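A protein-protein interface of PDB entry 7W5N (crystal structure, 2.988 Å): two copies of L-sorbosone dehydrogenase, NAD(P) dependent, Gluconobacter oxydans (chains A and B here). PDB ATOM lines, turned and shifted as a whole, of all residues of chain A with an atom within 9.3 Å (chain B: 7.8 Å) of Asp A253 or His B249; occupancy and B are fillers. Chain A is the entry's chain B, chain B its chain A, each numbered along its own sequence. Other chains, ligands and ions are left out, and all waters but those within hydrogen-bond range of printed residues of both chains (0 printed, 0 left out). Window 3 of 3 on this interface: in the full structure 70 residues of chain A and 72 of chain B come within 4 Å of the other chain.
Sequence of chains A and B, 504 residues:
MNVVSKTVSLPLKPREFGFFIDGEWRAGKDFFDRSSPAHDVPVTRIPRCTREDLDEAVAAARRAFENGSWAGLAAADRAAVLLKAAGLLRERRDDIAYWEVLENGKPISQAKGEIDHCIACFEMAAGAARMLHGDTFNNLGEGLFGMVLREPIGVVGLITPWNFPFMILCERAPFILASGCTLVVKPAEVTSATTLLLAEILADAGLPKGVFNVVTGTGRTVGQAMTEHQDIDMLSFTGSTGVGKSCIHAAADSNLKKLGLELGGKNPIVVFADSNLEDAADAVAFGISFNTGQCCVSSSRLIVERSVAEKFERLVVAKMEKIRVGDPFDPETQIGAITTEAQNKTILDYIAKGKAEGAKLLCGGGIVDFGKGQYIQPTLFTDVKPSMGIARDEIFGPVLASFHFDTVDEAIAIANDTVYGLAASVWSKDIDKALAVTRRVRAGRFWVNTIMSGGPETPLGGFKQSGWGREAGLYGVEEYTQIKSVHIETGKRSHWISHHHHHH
O of Ala B250 lies within hydrogen-bond range of OG of Ser B254.
OG of Ser B254 is in hydrogen-bond range of O of Ala B251, 3.2 Å away.
The backbone carbonyl oxygen (O) of Leu B261 is in hydrogen-bond range of the backbone NH (N) of Trp B468, at 2.8 Å.
O of Thr A227 lies within hydrogen-bond range of NZ of Lys A257 (3.0 Å).
NZ of Lys A257 sits at hydrogen-bond distance from O of His A229.
NZ of Lys A257 lies within hydrogen-bond range of OD1 of Asn A255 (2.8 Å).
Of the 19 printed residues of chain B, 8 touch a printed residue of chain A.
Hydrophobic or aromatic side chains of chain B within 4 Å of the printed part of chain A: Ile B248, His B249, Ala B252, Leu B259 and Trp B468.
Printed residues of chain A that touch a printed residue of chain B: Lys A245, Ile A248, His A249, Ala A252, Asp A253, Leu A256, Lys A257 and Trp A468.
Hydrophobic or aromatic side chains of chain A within 4 Å of the printed part of chain B: Ile A248, His A249, Ala A252, Leu A256 and Trp A468.
Among the printed residues, 16 pairs touch across the chains.
Among the printed residues, no Asp or Glu carboxylate lies within 4 Å of a Lys or Arg side-chain nitrogen of the other chain.
Asp A253 touches just one residue of chain B: His B249 (2.9 Å).
His B249 touches just these residues of chain A: His A249, Ala A252 and Asp A253.
Ala A252 touches just these residues of chain B: Lys B245 (3.2 Å), Ile B248 (3.5 Å) and His B249 (3.6 Å).
No residue of chain A comes within 4 Å of Ala B251.
Of chain A, only Lys A245 (3.5 Å), Ile A248 (3.5 Å) and His A249 (3.3 Å) come within 4 Å of Ala B252.
Of the printed residues of chain B, Ile A248 touches Ile B248 and Ala B252.
Printed residues of chain A within 4 Å of Leu B259: Trp A468 (3.9 Å).
Glu B228 touches none of the printed residues of chain A.
Leu B261 touches none of the printed residues of chain A.
The nearest residue of chain B that does not touch Asp A253 is Lys B245 (5.3 Å).
Lys A245 touches Ala B252, and with the chains exchanged Ala A252 touches Lys B245.
His A249 touches Ala B252, and with the chains exchanged Ala A252 touches His B249.
Trp A468 touches Leu B259, but with the chains exchanged Leu A259 does not touch Trp B468 (5.1 Å).
Trp A468 touches its own counterpart, Trp B468.
Of the 16 pairs that touch across the chains among the printed residues, 11 have their exchanged pair printed and touching as well.
Lys A245 touches Ser B254.
Ile A248 touches Ile B248.
Ile A248 touches Ala B252.
Ala B252 touches His A249.
Ala A252 touches Lys B245.
CG2 of Ile B248 touches CB of Ala A252, at 3.5 Å.
CG of Lys B245 touches CD1 of Leu A256, 3.99 Å away.
CZ2 of Trp B468 touches O of Lys A257 (3.4 Å).
CH2 of Trp A468 touches CD1 of Leu B259, 3.9 Å away.
CZ3 of Trp B468 touches CZ3 of Trp A468, at 3.5 Å.
A ring nitrogen (ND1) of His B249 lies within hydrogen-bond range of a ring nitrogen (ND1) of His A249 (2.6 Å).
OD1 of Asp A253 sits at hydrogen-bond distance from NE2 of His B249.
The side-chain carboxylate (OD1) of Asp B253 lies within hydrogen-bond range of a ring nitrogen (NE2) of His A249 (3.0 Å).
The indole nitrogen of Trp B468 is in hydrogen-bond range of the backbone carbonyl oxygen of Leu A256 (2.7 Å).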
ATOM      1  N   THR A 227      11.037 -33.708  28.818  1.00  0.00           N
ATOM      2  CA  THR A 227      10.029 -32.641  29.056  1.00  0.00           C
ATOM      3  C   THR A 227       9.636 -32.024  27.714  1.00  0.00           C
ATOM      4  O   THR A 227       8.505 -31.526  27.619  1.00  0.00           O
ATOM      5  CB  THR A 227      10.469 -31.575  30.081  1.00  0.00           C
ATOM      6  OG1 THR A 227      11.626 -30.831  29.672  1.00  0.00           O
ATOM      7  CG2 THR A 227      10.674 -32.181  31.458  1.00  0.00           C
ATOM      8  N   GLU A 228      10.505 -32.084  26.709  1.00  0.00           N
ATOM      9  CA  GLU A 228      10.254 -31.475  25.379  1.00  0.00           C
ATOM     10  C   GLU A 228       9.919 -32.543  24.335  1.00  0.00           C
ATOM     11  O   GLU A 228       9.548 -32.165  23.223  1.00  0.00           O
ATOM     12  CB  GLU A 228      11.496 -30.694  24.948  1.00  0.00           C
ATOM     13  CG  GLU A 228      11.766 -29.477  25.824  1.00  0.00           C
ATOM     14  CD  GLU A 228      12.976 -28.674  25.385  1.00  0.00           C
ATOM     15  OE1 GLU A 228      13.710 -29.151  24.491  1.00  0.00           O
ATOM     16  OE2 GLU A 228      13.180 -27.583  25.924  1.00  0.00           O
ATOM     17  N   HIS A 229      10.068 -33.823  24.666  1.00  0.00           N
ATOM     18  CA  HIS A 229       9.927 -34.940  23.697  1.00  0.00           C
ATOM     19  C   HIS A 229       8.589 -34.859  22.971  1.00  0.00           C
ATOM     20  O   HIS A 229       7.590 -34.641  23.645  1.00  0.00           O
ATOM     21  CB  HIS A 229      10.040 -36.311  24.353  1.00  0.00           C
ATOM     22  CG  HIS A 229      10.511 -37.315  23.371  1.00  0.00           C
ATOM     23  ND1 HIS A 229       9.653 -37.937  22.495  1.00  0.00           N
ATOM     24  CD2 HIS A 229      11.756 -37.715  23.053  1.00  0.00           C
ATOM     25  CE1 HIS A 229      10.342 -38.724  21.705  1.00  0.00           C
ATOM     26  NE2 HIS A 229      11.634 -38.600  22.023  1.00  0.00           N
ATOM     27  N   GLN A 230       8.579 -35.106  21.662  1.00  0.00           N
ATOM     28  CA  GLN A 230       7.374 -34.882  20.833  1.00  0.00           C
ATOM     29  C   GLN A 230       6.461 -36.112  20.843  1.00  0.00           C
ATOM     30  O   GLN A 230       5.341 -35.992  20.263  1.00  0.00           O
ATOM     31  CB  GLN A 230       7.757 -34.464  19.412  1.00  0.00           C
ATOM     32  CG  GLN A 230       6.790 -33.438  18.786  1.00  0.00           C
ATOM     33  CD  GLN A 230       6.867 -32.042  19.368  1.00  0.00           C
ATOM     34  OE1 GLN A 230       7.429 -31.806  20.433  1.00  0.00           O
ATOM     35  NE2 GLN A 230       6.291 -31.080  18.677  1.00  0.00           N
ATOM     36  N   LYS A 245       7.969 -25.843  36.803  1.00  0.00           N
ATOM     37  CA  LYS A 245       7.622 -24.695  35.923  1.00  0.00           C
ATOM     38  C   LYS A 245       8.369 -24.840  34.588  1.00  0.00           C
ATOM     39  O   LYS A 245       7.805 -24.395  33.567  1.00  0.00           O
ATOM     40  CB  LYS A 245       7.905 -23.371  36.648  1.00  0.00           C
ATOM     41  CG  LYS A 245       7.068 -23.129  37.904  1.00  0.00           C
ATOM     42  CD  LYS A 245       7.341 -21.826  38.646  1.00  0.00           C
ATOM     43  CE  LYS A 245       6.143 -21.387  39.475  1.00  0.00           C
ATOM     44  NZ  LYS A 245       5.976 -19.907  39.521  1.00  0.00           N
ATOM     45  N   SER A 246       9.573 -25.435  34.593  1.00  0.00           N
ATOM     46  CA  SER A 246      10.377 -25.779  33.381  1.00  0.00           C
ATOM     47  C   SER A 246       9.667 -26.842  32.538  1.00  0.00           C
ATOM     48  O   SER A 246       9.664 -26.742  31.304  1.00  0.00           O
ATOM     49  CB  SER A 246      11.739 -26.281  33.764  1.00  0.00           C
ATOM     50  OG  SER A 246      12.528 -25.238  34.298  1.00  0.00           O
ATOM     51  N   CYS A 247       9.145 -27.863  33.215  1.00  0.00           N
ATOM     52  CA  CYS A 247       8.408 -29.002  32.622  1.00  0.00           C
ATOM     53  C   CYS A 247       7.181 -28.466  31.884  1.00  0.00           C
ATOM     54  O   CYS A 247       6.898 -29.007  30.779  1.00  0.00           O
ATOM     55  CB  CYS A 247       7.960 -30.009  33.680  1.00  0.00           C
ATOM     56  SG  CYS A 247       9.297 -30.890  34.539  1.00  0.00           S
ATOM     57  N   ILE A 248       6.485 -27.488  32.505  1.00  0.00           N
ATOM     58  CA  ILE A 248       5.230 -26.841  31.999  1.00  0.00           C
ATOM     59  C   ILE A 248       5.566 -26.080  30.714  1.00  0.00           C
ATOM     60  O   ILE A 248       4.935 -26.334  29.693  1.00  0.00           O
ATOM     61  CB  ILE A 248       4.572 -25.919  33.055  1.00  0.00           C
ATOM     62  CG1 ILE A 248       4.217 -26.682  34.334  1.00  0.00           C
ATOM     63  CG2 ILE A 248       3.358 -25.196  32.461  1.00  0.00           C
ATOM     64  CD1 ILE A 248       3.431 -25.885  35.351  1.00  0.00           C
ATOM     65  N   HIS A 249       6.545 -25.184  30.771  1.00  0.00           N
ATOM     66  CA  HIS A 249       7.018 -24.415  29.593  1.00  0.00           C
ATOM     67  C   HIS A 249       7.315 -25.388  28.442  1.00  0.00           C
ATOM     68  O   HIS A 249       6.817 -25.158  27.307  1.00  0.00           O
ATOM     69  CB  HIS A 249       8.208 -23.528  29.983  1.00  0.00           C
ATOM     70  CG  HIS A 249       7.795 -22.273  30.679  1.00  0.00           C
ATOM     71  ND1 HIS A 249       7.043 -21.293  30.046  1.00  0.00           N
ATOM     72  CD2 HIS A 249       8.008 -21.839  31.945  1.00  0.00           C
ATOM     73  CE1 HIS A 249       6.812 -20.316  30.900  1.00  0.00           C
ATOM     74  NE2 HIS A 249       7.396 -20.620  32.075  1.00  0.00           N
ATOM     75  N   ALA A 250       8.065 -26.457  28.742  1.00  0.00           N
ATOM     76  CA  ALA A 250       8.488 -27.514  27.789  1.00  0.00           C
ATOM     77  C   ALA A 250       7.253 -28.180  27.168  1.00  0.00           C
ATOM     78  O   ALA A 250       7.265 -28.361  25.950  1.00  0.00           O
ATOM     79  CB  ALA A 250       9.393 -28.512  28.481  1.00  0.00           C
ATOM     80  N   ALA A 251       6.240 -28.511  27.977  1.00  0.00           N
ATOM     81  CA  ALA A 251       4.971 -29.135  27.540  1.00  0.00           C
ATOM     82  C   ALA A 251       4.305 -28.257  26.478  1.00  0.00           C
ATOM     83  O   ALA A 251       4.106 -28.737  25.349  1.00  0.00           O
ATOM     84  CB  ALA A 251       4.055 -29.362  28.716  1.00  0.00           C
ATOM     85  N   ALA A 252       3.970 -27.015  26.837  1.00  0.00           N
ATOM     86  CA  ALA A 252       3.416 -25.989  25.918  1.00  0.00           C
ATOM     87  C   ALA A 252       4.283 -25.896  24.667  1.00  0.00           C
ATOM     88  O   ALA A 252       3.706 -25.850  23.586  1.00  0.00           O
ATOM     89  CB  ALA A 252       3.360 -24.635  26.582  1.00  0.00           C
ATOM     90  N   ASP A 253       5.609 -25.842  24.829  1.00  0.00           N
ATOM     91  CA  ASP A 253       6.569 -25.613  23.723  1.00  0.00           C
ATOM     92  C   ASP A 253       6.761 -26.890  22.898  1.00  0.00           C
ATOM     93  O   ASP A 253       7.471 -26.818  21.904  1.00  0.00           O
ATOM     94  CB  ASP A 253       7.906 -25.048  24.231  1.00  0.00           C
ATOM     95  CG  ASP A 253       7.971 -23.529  24.148  1.00  0.00           C
ATOM     96  OD1 ASP A 253       7.106 -22.962  23.435  1.00  0.00           O
ATOM     97  OD2 ASP A 253       8.850 -22.911  24.812  1.00  0.00           O
ATOM     98  N   SER A 254       6.179 -28.022  23.254  1.00  0.00           N
ATOM     99  CA  SER A 254       6.417 -29.293  22.522  1.00  0.00           C
ATOM    100  C   SER A 254       5.095 -29.828  21.954  1.00  0.00           C
ATOM    101  O   SER A 254       4.705 -29.323  20.875  1.00  0.00           O
ATOM    102  CB  SER A 254       7.149 -30.306  23.382  1.00  0.00           C
ATOM    103  OG  SER A 254       6.477 -30.584  24.598  1.00  0.00           O
ATOM    104  N   ASN A 255       4.417 -30.743  22.679  1.00  0.00           N
ATOM    105  CA  ASN A 255       3.243 -31.539  22.213  1.00  0.00           C
ATOM    106  C   ASN A 255       2.053 -31.502  23.176  1.00  0.00           C
ATOM    107  O   ASN A 255       1.208 -32.370  23.029  1.00  0.00           O
ATOM    108  CB  ASN A 255       3.579 -33.023  22.040  1.00  0.00           C
ATOM    109  CG  ASN A 255       3.978 -33.718  23.323  1.00  0.00           C
ATOM    110  OD1 ASN A 255       4.601 -33.128  24.184  1.00  0.00           O
ATOM    111  ND2 ASN A 255       3.697 -34.997  23.439  1.00  0.00           N
ATOM    112  N   LEU A 256       1.974 -30.545  24.104  1.00  0.00           N
ATOM    113  CA  LEU A 256       0.815 -30.336  25.031  1.00  0.00           C
ATOM    114  C   LEU A 256       0.627 -31.561  25.939  1.00  0.00           C
ATOM    115  O   LEU A 256      -0.475 -31.764  26.492  1.00  0.00           O
ATOM    116  CB  LEU A 256      -0.443 -30.046  24.204  1.00  0.00           C
ATOM    117  CG  LEU A 256      -1.411 -29.018  24.803  1.00  0.00           C
ATOM    118  CD1 LEU A 256      -1.603 -27.838  23.838  1.00  0.00           C
ATOM    119  CD2 LEU A 256      -2.749 -29.679  25.138  1.00  0.00           C
ATOM    120  N   LYS A 257       1.688 -32.345  26.092  1.00  0.00           N
ATOM    121  CA  LYS A 257       1.707 -33.557  26.935  1.00  0.00           C
ATOM    122  C   LYS A 257       1.113 -33.164  28.289  1.00  0.00           C
ATOM    123  O   LYS A 257       1.311 -32.025  28.716  1.00  0.00           O
ATOM    124  CB  LYS A 257       3.142 -34.104  27.044  1.00  0.00           C
ATOM    125  CG  LYS A 257       4.133 -33.245  27.838  1.00  0.00           C
ATOM    126  CD  LYS A 257       5.395 -33.969  28.217  1.00  0.00           C
ATOM    127  CE  LYS A 257       6.170 -34.454  27.018  1.00  0.00           C
ATOM    128  NZ  LYS A 257       6.607 -33.320  26.184  1.00  0.00           N
ATOM    129  N   LEU A 259       0.662 -33.229  32.434  1.00  0.00           N
ATOM    130  CA  LEU A 259       1.675 -33.111  33.505  1.00  0.00           C
ATOM    131  C   LEU A 259       1.046 -33.455  34.844  1.00  0.00           C
ATOM    132  O   LEU A 259       0.088 -32.771  35.231  1.00  0.00           O
ATOM    133  CB  LEU A 259       2.218 -31.683  33.540  1.00  0.00           C
ATOM    134  CG  LEU A 259       3.215 -31.339  32.436  1.00  0.00           C
ATOM    135  CD1 LEU A 259       3.799 -29.953  32.675  1.00  0.00           C
ATOM    136  CD2 LEU A 259       4.322 -32.393  32.356  1.00  0.00           C
ATOM    137  N   TRP A 468       0.057 -30.353  40.273  1.00  0.00           N
ATOM    138  CA  TRP A 468      -1.132 -30.692  39.451  1.00  0.00           C
ATOM    139  C   TRP A 468      -1.409 -32.189  39.545  1.00  0.00           C
ATOM    140  O   TRP A 468      -0.435 -32.985  39.475  1.00  0.00           O
ATOM    141  CB  TRP A 468      -0.925 -30.318  37.982  1.00  0.00           C
ATOM    142  CG  TRP A 468      -0.856 -28.862  37.663  1.00  0.00           C
ATOM    143  CD1 TRP A 468      -1.194 -27.802  38.456  1.00  0.00           C
ATOM    144  CD2 TRP A 468      -0.483 -28.310  36.392  1.00  0.00           C
ATOM    145  NE1 TRP A 468      -1.021 -26.622  37.774  1.00  0.00           N
ATOM    146  CE2 TRP A 468      -0.582 -26.905  36.506  1.00  0.00           C
ATOM    147  CE3 TRP A 468      -0.057 -28.860  35.182  1.00  0.00           C
ATOM    148  CZ2 TRP A 468      -0.263 -26.056  35.445  1.00  0.00           C
ATOM    149  CZ3 TRP A 468       0.266 -28.019  34.142  1.00  0.00           C
ATOM    150  CH2 TRP A 468       0.149 -26.636  34.265  1.00  0.00           C
ATOM    151  N   THR B 227      -4.617 -15.018  32.304  1.00  0.00           N
ATOM    152  CA  THR B 227      -3.744 -16.214  32.233  1.00  0.00           C
ATOM    153  C   THR B 227      -2.541 -16.025  33.171  1.00  0.00           C
ATOM    154  O   THR B 227      -2.073 -17.035  33.697  1.00  0.00           O
ATOM    155  CB  THR B 227      -3.371 -16.603  30.794  1.00  0.00           C
ATOM    156  OG1 THR B 227      -2.634 -15.561  30.169  1.00  0.00           O
ATOM    157  CG2 THR B 227      -4.578 -16.953  29.956  1.00  0.00           C
ATOM    158  N   GLU B 228      -2.078 -14.795  33.423  1.00  0.00           N
ATOM    159  CA  GLU B 228      -0.888 -14.568  34.294  1.00  0.00           C
ATOM    160  C   GLU B 228      -1.298 -13.955  35.640  1.00  0.00           C
ATOM    161  O   GLU B 228      -0.414 -13.751  36.486  1.00  0.00           O
ATOM    162  CB  GLU B 228       0.230 -13.802  33.558  1.00  0.00           C
ATOM    163  CG  GLU B 228      -0.103 -12.420  33.003  1.00  0.00           C
ATOM    164  CD  GLU B 228       0.909 -11.850  31.991  1.00  0.00           C
ATOM    165  OE1 GLU B 228       0.714 -10.677  31.529  1.00  0.00           O
ATOM    166  OE2 GLU B 228       1.900 -12.566  31.634  1.00  0.00           O
ATOM    167  N   GLY B 242      -2.926 -22.940  19.767  1.00  0.00           N
ATOM    168  CA  GLY B 242      -1.908 -21.874  19.844  1.00  0.00           C
ATOM    169  C   GLY B 242      -2.090 -20.975  21.057  1.00  0.00           C
ATOM    170  O   GLY B 242      -1.091 -20.627  21.718  1.00  0.00           O
ATOM    171  N   VAL B 243      -3.320 -20.605  21.372  1.00  0.00           N
ATOM    172  CA  VAL B 243      -3.593 -19.743  22.547  1.00  0.00           C
ATOM    173  C   VAL B 243      -3.556 -20.621  23.798  1.00  0.00           C
ATOM    174  O   VAL B 243      -3.124 -20.138  24.845  1.00  0.00           O
ATOM    175  CB  VAL B 243      -4.926 -18.998  22.367  1.00  0.00           C
ATOM    176  CG1 VAL B 243      -5.172 -17.974  23.473  1.00  0.00           C
ATOM    177  CG2 VAL B 243      -4.940 -18.317  21.013  1.00  0.00           C
ATOM    178  N   GLY B 244      -3.991 -21.867  23.680  1.00  0.00           N
ATOM    179  CA  GLY B 244      -3.855 -22.859  24.760  1.00  0.00           C
ATOM    180  C   GLY B 244      -2.415 -22.961  25.241  1.00  0.00           C
ATOM    181  O   GLY B 244      -2.203 -22.917  26.481  1.00  0.00           O
ATOM    182  N   LYS B 245      -1.458 -23.083  24.312  1.00  0.00           N
ATOM    183  CA  LYS B 245      -0.004 -23.078  24.635  1.00  0.00           C
ATOM    184  C   LYS B 245       0.398 -21.766  25.342  1.00  0.00           C
ATOM    185  O   LYS B 245       1.228 -21.829  26.291  1.00  0.00           O
ATOM    186  CB  LYS B 245       0.806 -23.341  23.367  1.00  0.00           C
ATOM    187  CG  LYS B 245       0.785 -24.784  22.880  1.00  0.00           C
ATOM    188  CD  LYS B 245       1.273 -24.936  21.450  1.00  0.00           C
ATOM    189  CE  LYS B 245       1.342 -26.367  20.960  1.00  0.00           C
ATOM    190  NZ  LYS B 245       1.081 -26.446  19.499  1.00  0.00           N
ATOM    191  N   SER B 246      -0.160 -20.625  24.920  1.00  0.00           N
ATOM    192  CA  SER B 246       0.004 -19.302  25.583  1.00  0.00           C
ATOM    193  C   SER B 246      -0.436 -19.371  27.048  1.00  0.00           C
ATOM    194  O   SER B 246       0.307 -18.868  27.917  1.00  0.00           O
ATOM    195  CB  SER B 246      -0.759 -18.227  24.866  1.00  0.00           C
ATOM    196  OG  SER B 246      -0.088 -17.853  23.676  1.00  0.00           O
ATOM    197  N   CYS B 247      -1.618 -19.941  27.301  1.00  0.00           N
ATOM    198  CA  CYS B 247      -2.218 -20.101  28.653  1.00  0.00           C
ATOM    199  C   CYS B 247      -1.293 -20.989  29.488  1.00  0.00           C
ATOM    200  O   CYS B 247      -1.087 -20.687  30.670  1.00  0.00           O
ATOM    201  CB  CYS B 247      -3.621 -20.706  28.600  1.00  0.00           C
ATOM    202  SG  CYS B 247      -4.888 -19.670  27.804  1.00  0.00           S
ATOM    203  N   ILE B 248      -0.731 -22.039  28.898  1.00  0.00           N
ATOM    204  CA  ILE B 248       0.145 -22.989  29.641  1.00  0.00           C
ATOM    205  C   ILE B 248       1.383 -22.226  30.113  1.00  0.00           C
ATOM    206  O   ILE B 248       1.635 -22.230  31.321  1.00  0.00           O
ATOM    207  CB  ILE B 248       0.481 -24.231  28.794  1.00  0.00           C
ATOM    208  CG1 ILE B 248      -0.787 -25.019  28.463  1.00  0.00           C
ATOM    209  CG2 ILE B 248       1.495 -25.111  29.506  1.00  0.00           C
ATOM    210  CD1 ILE B 248      -0.597 -26.078  27.414  1.00  0.00           C
ATOM    211  N   HIS B 249       2.113 -21.592  29.191  1.00  0.00           N
ATOM    212  CA  HIS B 249       3.270 -20.694  29.478  1.00  0.00           C
ATOM    213  C   HIS B 249       2.904 -19.668  30.563  1.00  0.00           C
ATOM    214  O   HIS B 249       3.645 -19.556  31.536  1.00  0.00           O
ATOM    215  CB  HIS B 249       3.737 -19.997  28.184  1.00  0.00           C
ATOM    216  CG  HIS B 249       4.600 -20.846  27.314  1.00  0.00           C
ATOM    217  ND1 HIS B 249       5.777 -21.409  27.779  1.00  0.00           N
ATOM    218  CD2 HIS B 249       4.486 -21.198  26.017  1.00  0.00           C
ATOM    219  CE1 HIS B 249       6.344 -22.090  26.799  1.00  0.00           C
ATOM    220  NE2 HIS B 249       5.572 -21.976  25.706  1.00  0.00           N
ATOM    221  N   ALA B 250       1.800 -18.937  30.377  1.00  0.00           N
ATOM    222  CA  ALA B 250       1.306 -17.890  31.307  1.00  0.00           C
ATOM    223  C   ALA B 250       1.181 -18.462  32.718  1.00  0.00           C
ATOM    224  O   ALA B 250       1.609 -17.790  33.667  1.00  0.00           O
ATOM    225  CB  ALA B 250      -0.015 -17.338  30.833  1.00  0.00           C
ATOM    226  N   ALA B 251       0.601 -19.658  32.825  1.00  0.00           N
ATOM    227  CA  ALA B 251       0.402 -20.389  34.091  1.00  0.00           C
ATOM    228  C   ALA B 251       1.761 -20.653  34.759  1.00  0.00           C
ATOM    229  O   ALA B 251       1.893 -20.296  35.937  1.00  0.00           O
ATOM    230  CB  ALA B 251      -0.397 -21.638  33.838  1.00  0.00           C
ATOM    231  N   ALA B 252       2.757 -21.189  34.046  1.00  0.00           N
ATOM    232  CA  ALA B 252       4.109 -21.488  34.588  1.00  0.00           C
ATOM    233  C   ALA B 252       4.835 -20.208  35.056  1.00  0.00           C
ATOM    234  O   ALA B 252       5.598 -20.291  36.049  1.00  0.00           O
ATOM    235  CB  ALA B 252       4.936 -22.217  33.556  1.00  0.00           C
ATOM    236  N   ASP B 253       4.649 -19.078  34.358  1.00  0.00           N
ATOM    237  CA  ASP B 253       5.294 -17.770  34.666  1.00  0.00           C
ATOM    238  C   ASP B 253       4.518 -17.005  35.742  1.00  0.00           C
ATOM    239  O   ASP B 253       5.038 -15.946  36.161  1.00  0.00           O
ATOM    240  CB  ASP B 253       5.312 -16.834  33.462  1.00  0.00           C
ATOM    241  CG  ASP B 253       6.255 -17.271  32.365  1.00  0.00           C
ATOM    242  OD1 ASP B 253       7.370 -17.715  32.717  1.00  0.00           O
ATOM    243  OD2 ASP B 253       5.857 -17.162  31.158  1.00  0.00           O
ATOM    244  N   SER B 254       3.312 -17.465  36.118  1.00  0.00           N
ATOM    245  CA  SER B 254       2.449 -16.788  37.118  1.00  0.00           C
ATOM    246  C   SER B 254       2.432 -17.601  38.407  1.00  0.00           C
ATOM    247  O   SER B 254       3.455 -17.510  39.100  1.00  0.00           O
ATOM    248  CB  SER B 254       1.078 -16.484  36.586  1.00  0.00           C
ATOM    249  OG  SER B 254       0.290 -17.643  36.499  1.00  0.00           O
ATOM    250  N   ASN B 255       1.357 -18.353  38.697  1.00  0.00           N
ATOM    251  CA  ASN B 255       1.075 -18.951  40.040  1.00  0.00           C
ATOM    252  C   ASN B 255       0.850 -20.471  39.972  1.00  0.00           C
ATOM    253  O   ASN B 255       0.218 -20.992  40.905  1.00  0.00           O
ATOM    254  CB  ASN B 255      -0.140 -18.291  40.714  1.00  0.00           C
ATOM    255  CG  ASN B 255      -1.435 -18.401  39.930  1.00  0.00           C
ATOM    256  OD1 ASN B 255      -1.434 -18.872  38.798  1.00  0.00           O
ATOM    257  ND2 ASN B 255      -2.541 -17.953  40.510  1.00  0.00           N
ATOM    258  N   LEU B 259      -5.304 -25.583  34.507  1.00  0.00           N
ATOM    259  CA  LEU B 259      -5.899 -25.170  33.220  1.00  0.00           C
ATOM    260  C   LEU B 259      -6.888 -26.232  32.762  1.00  0.00           C
ATOM    261  O   LEU B 259      -6.505 -27.403  32.629  1.00  0.00           O
ATOM    262  CB  LEU B 259      -4.800 -24.981  32.172  1.00  0.00           C
ATOM    263  CG  LEU B 259      -3.674 -24.031  32.577  1.00  0.00           C
ATOM    264  CD1 LEU B 259      -2.329 -24.519  32.059  1.00  0.00           C
ATOM    265  CD2 LEU B 259      -3.954 -22.600  32.125  1.00  0.00           C
ATOM    266  N   LEU B 261      -8.254 -26.843  29.358  1.00  0.00           N
ATOM    267  CA  LEU B 261      -8.067 -26.400  27.967  1.00  0.00           C
ATOM    268  C   LEU B 261      -8.871 -27.288  27.017  1.00  0.00           C
ATOM    269  O   LEU B 261      -8.606 -28.492  26.984  1.00  0.00           O
ATOM    270  CB  LEU B 261      -6.575 -26.439  27.667  1.00  0.00           C
ATOM    271  CG  LEU B 261      -5.701 -25.672  28.655  1.00  0.00           C
ATOM    272  CD1 LEU B 261      -4.219 -25.838  28.307  1.00  0.00           C
ATOM    273  CD2 LEU B 261      -6.084 -24.203  28.682  1.00  0.00           C
ATOM    274  N   TRP B 468      -6.664 -30.272  27.858  1.00  0.00           N
ATOM    275  CA  TRP B 468      -6.573 -30.900  29.195  1.00  0.00           C
ATOM    276  C   TRP B 468      -7.914 -30.800  29.913  1.00  0.00           C
ATOM    277  O   TRP B 468      -8.531 -29.723  29.902  1.00  0.00           O
ATOM    278  CB  TRP B 468      -5.498 -30.230  30.040  1.00  0.00           C
ATOM    279  CG  TRP B 468      -4.112 -30.295  29.493  1.00  0.00           C
ATOM    280  CD1 TRP B 468      -3.617 -31.103  28.511  1.00  0.00           C
ATOM    281  CD2 TRP B 468      -2.999 -29.543  29.980  1.00  0.00           C
ATOM    282  NE1 TRP B 468      -2.277 -30.870  28.323  1.00  0.00           N
ATOM    283  CE2 TRP B 468      -1.873 -29.922  29.216  1.00  0.00           C
ATOM    284  CE3 TRP B 468      -2.857 -28.589  30.987  1.00  0.00           C
ATOM    285  CZ2 TRP B 468      -0.620 -29.363  29.415  1.00  0.00           C
ATOM    286  CZ3 TRP B 468      -1.617 -28.030  31.180  1.00  0.00           C
ATOM    287  CH2 TRP B 468      -0.515 -28.419  30.411  1.00  0.00           C
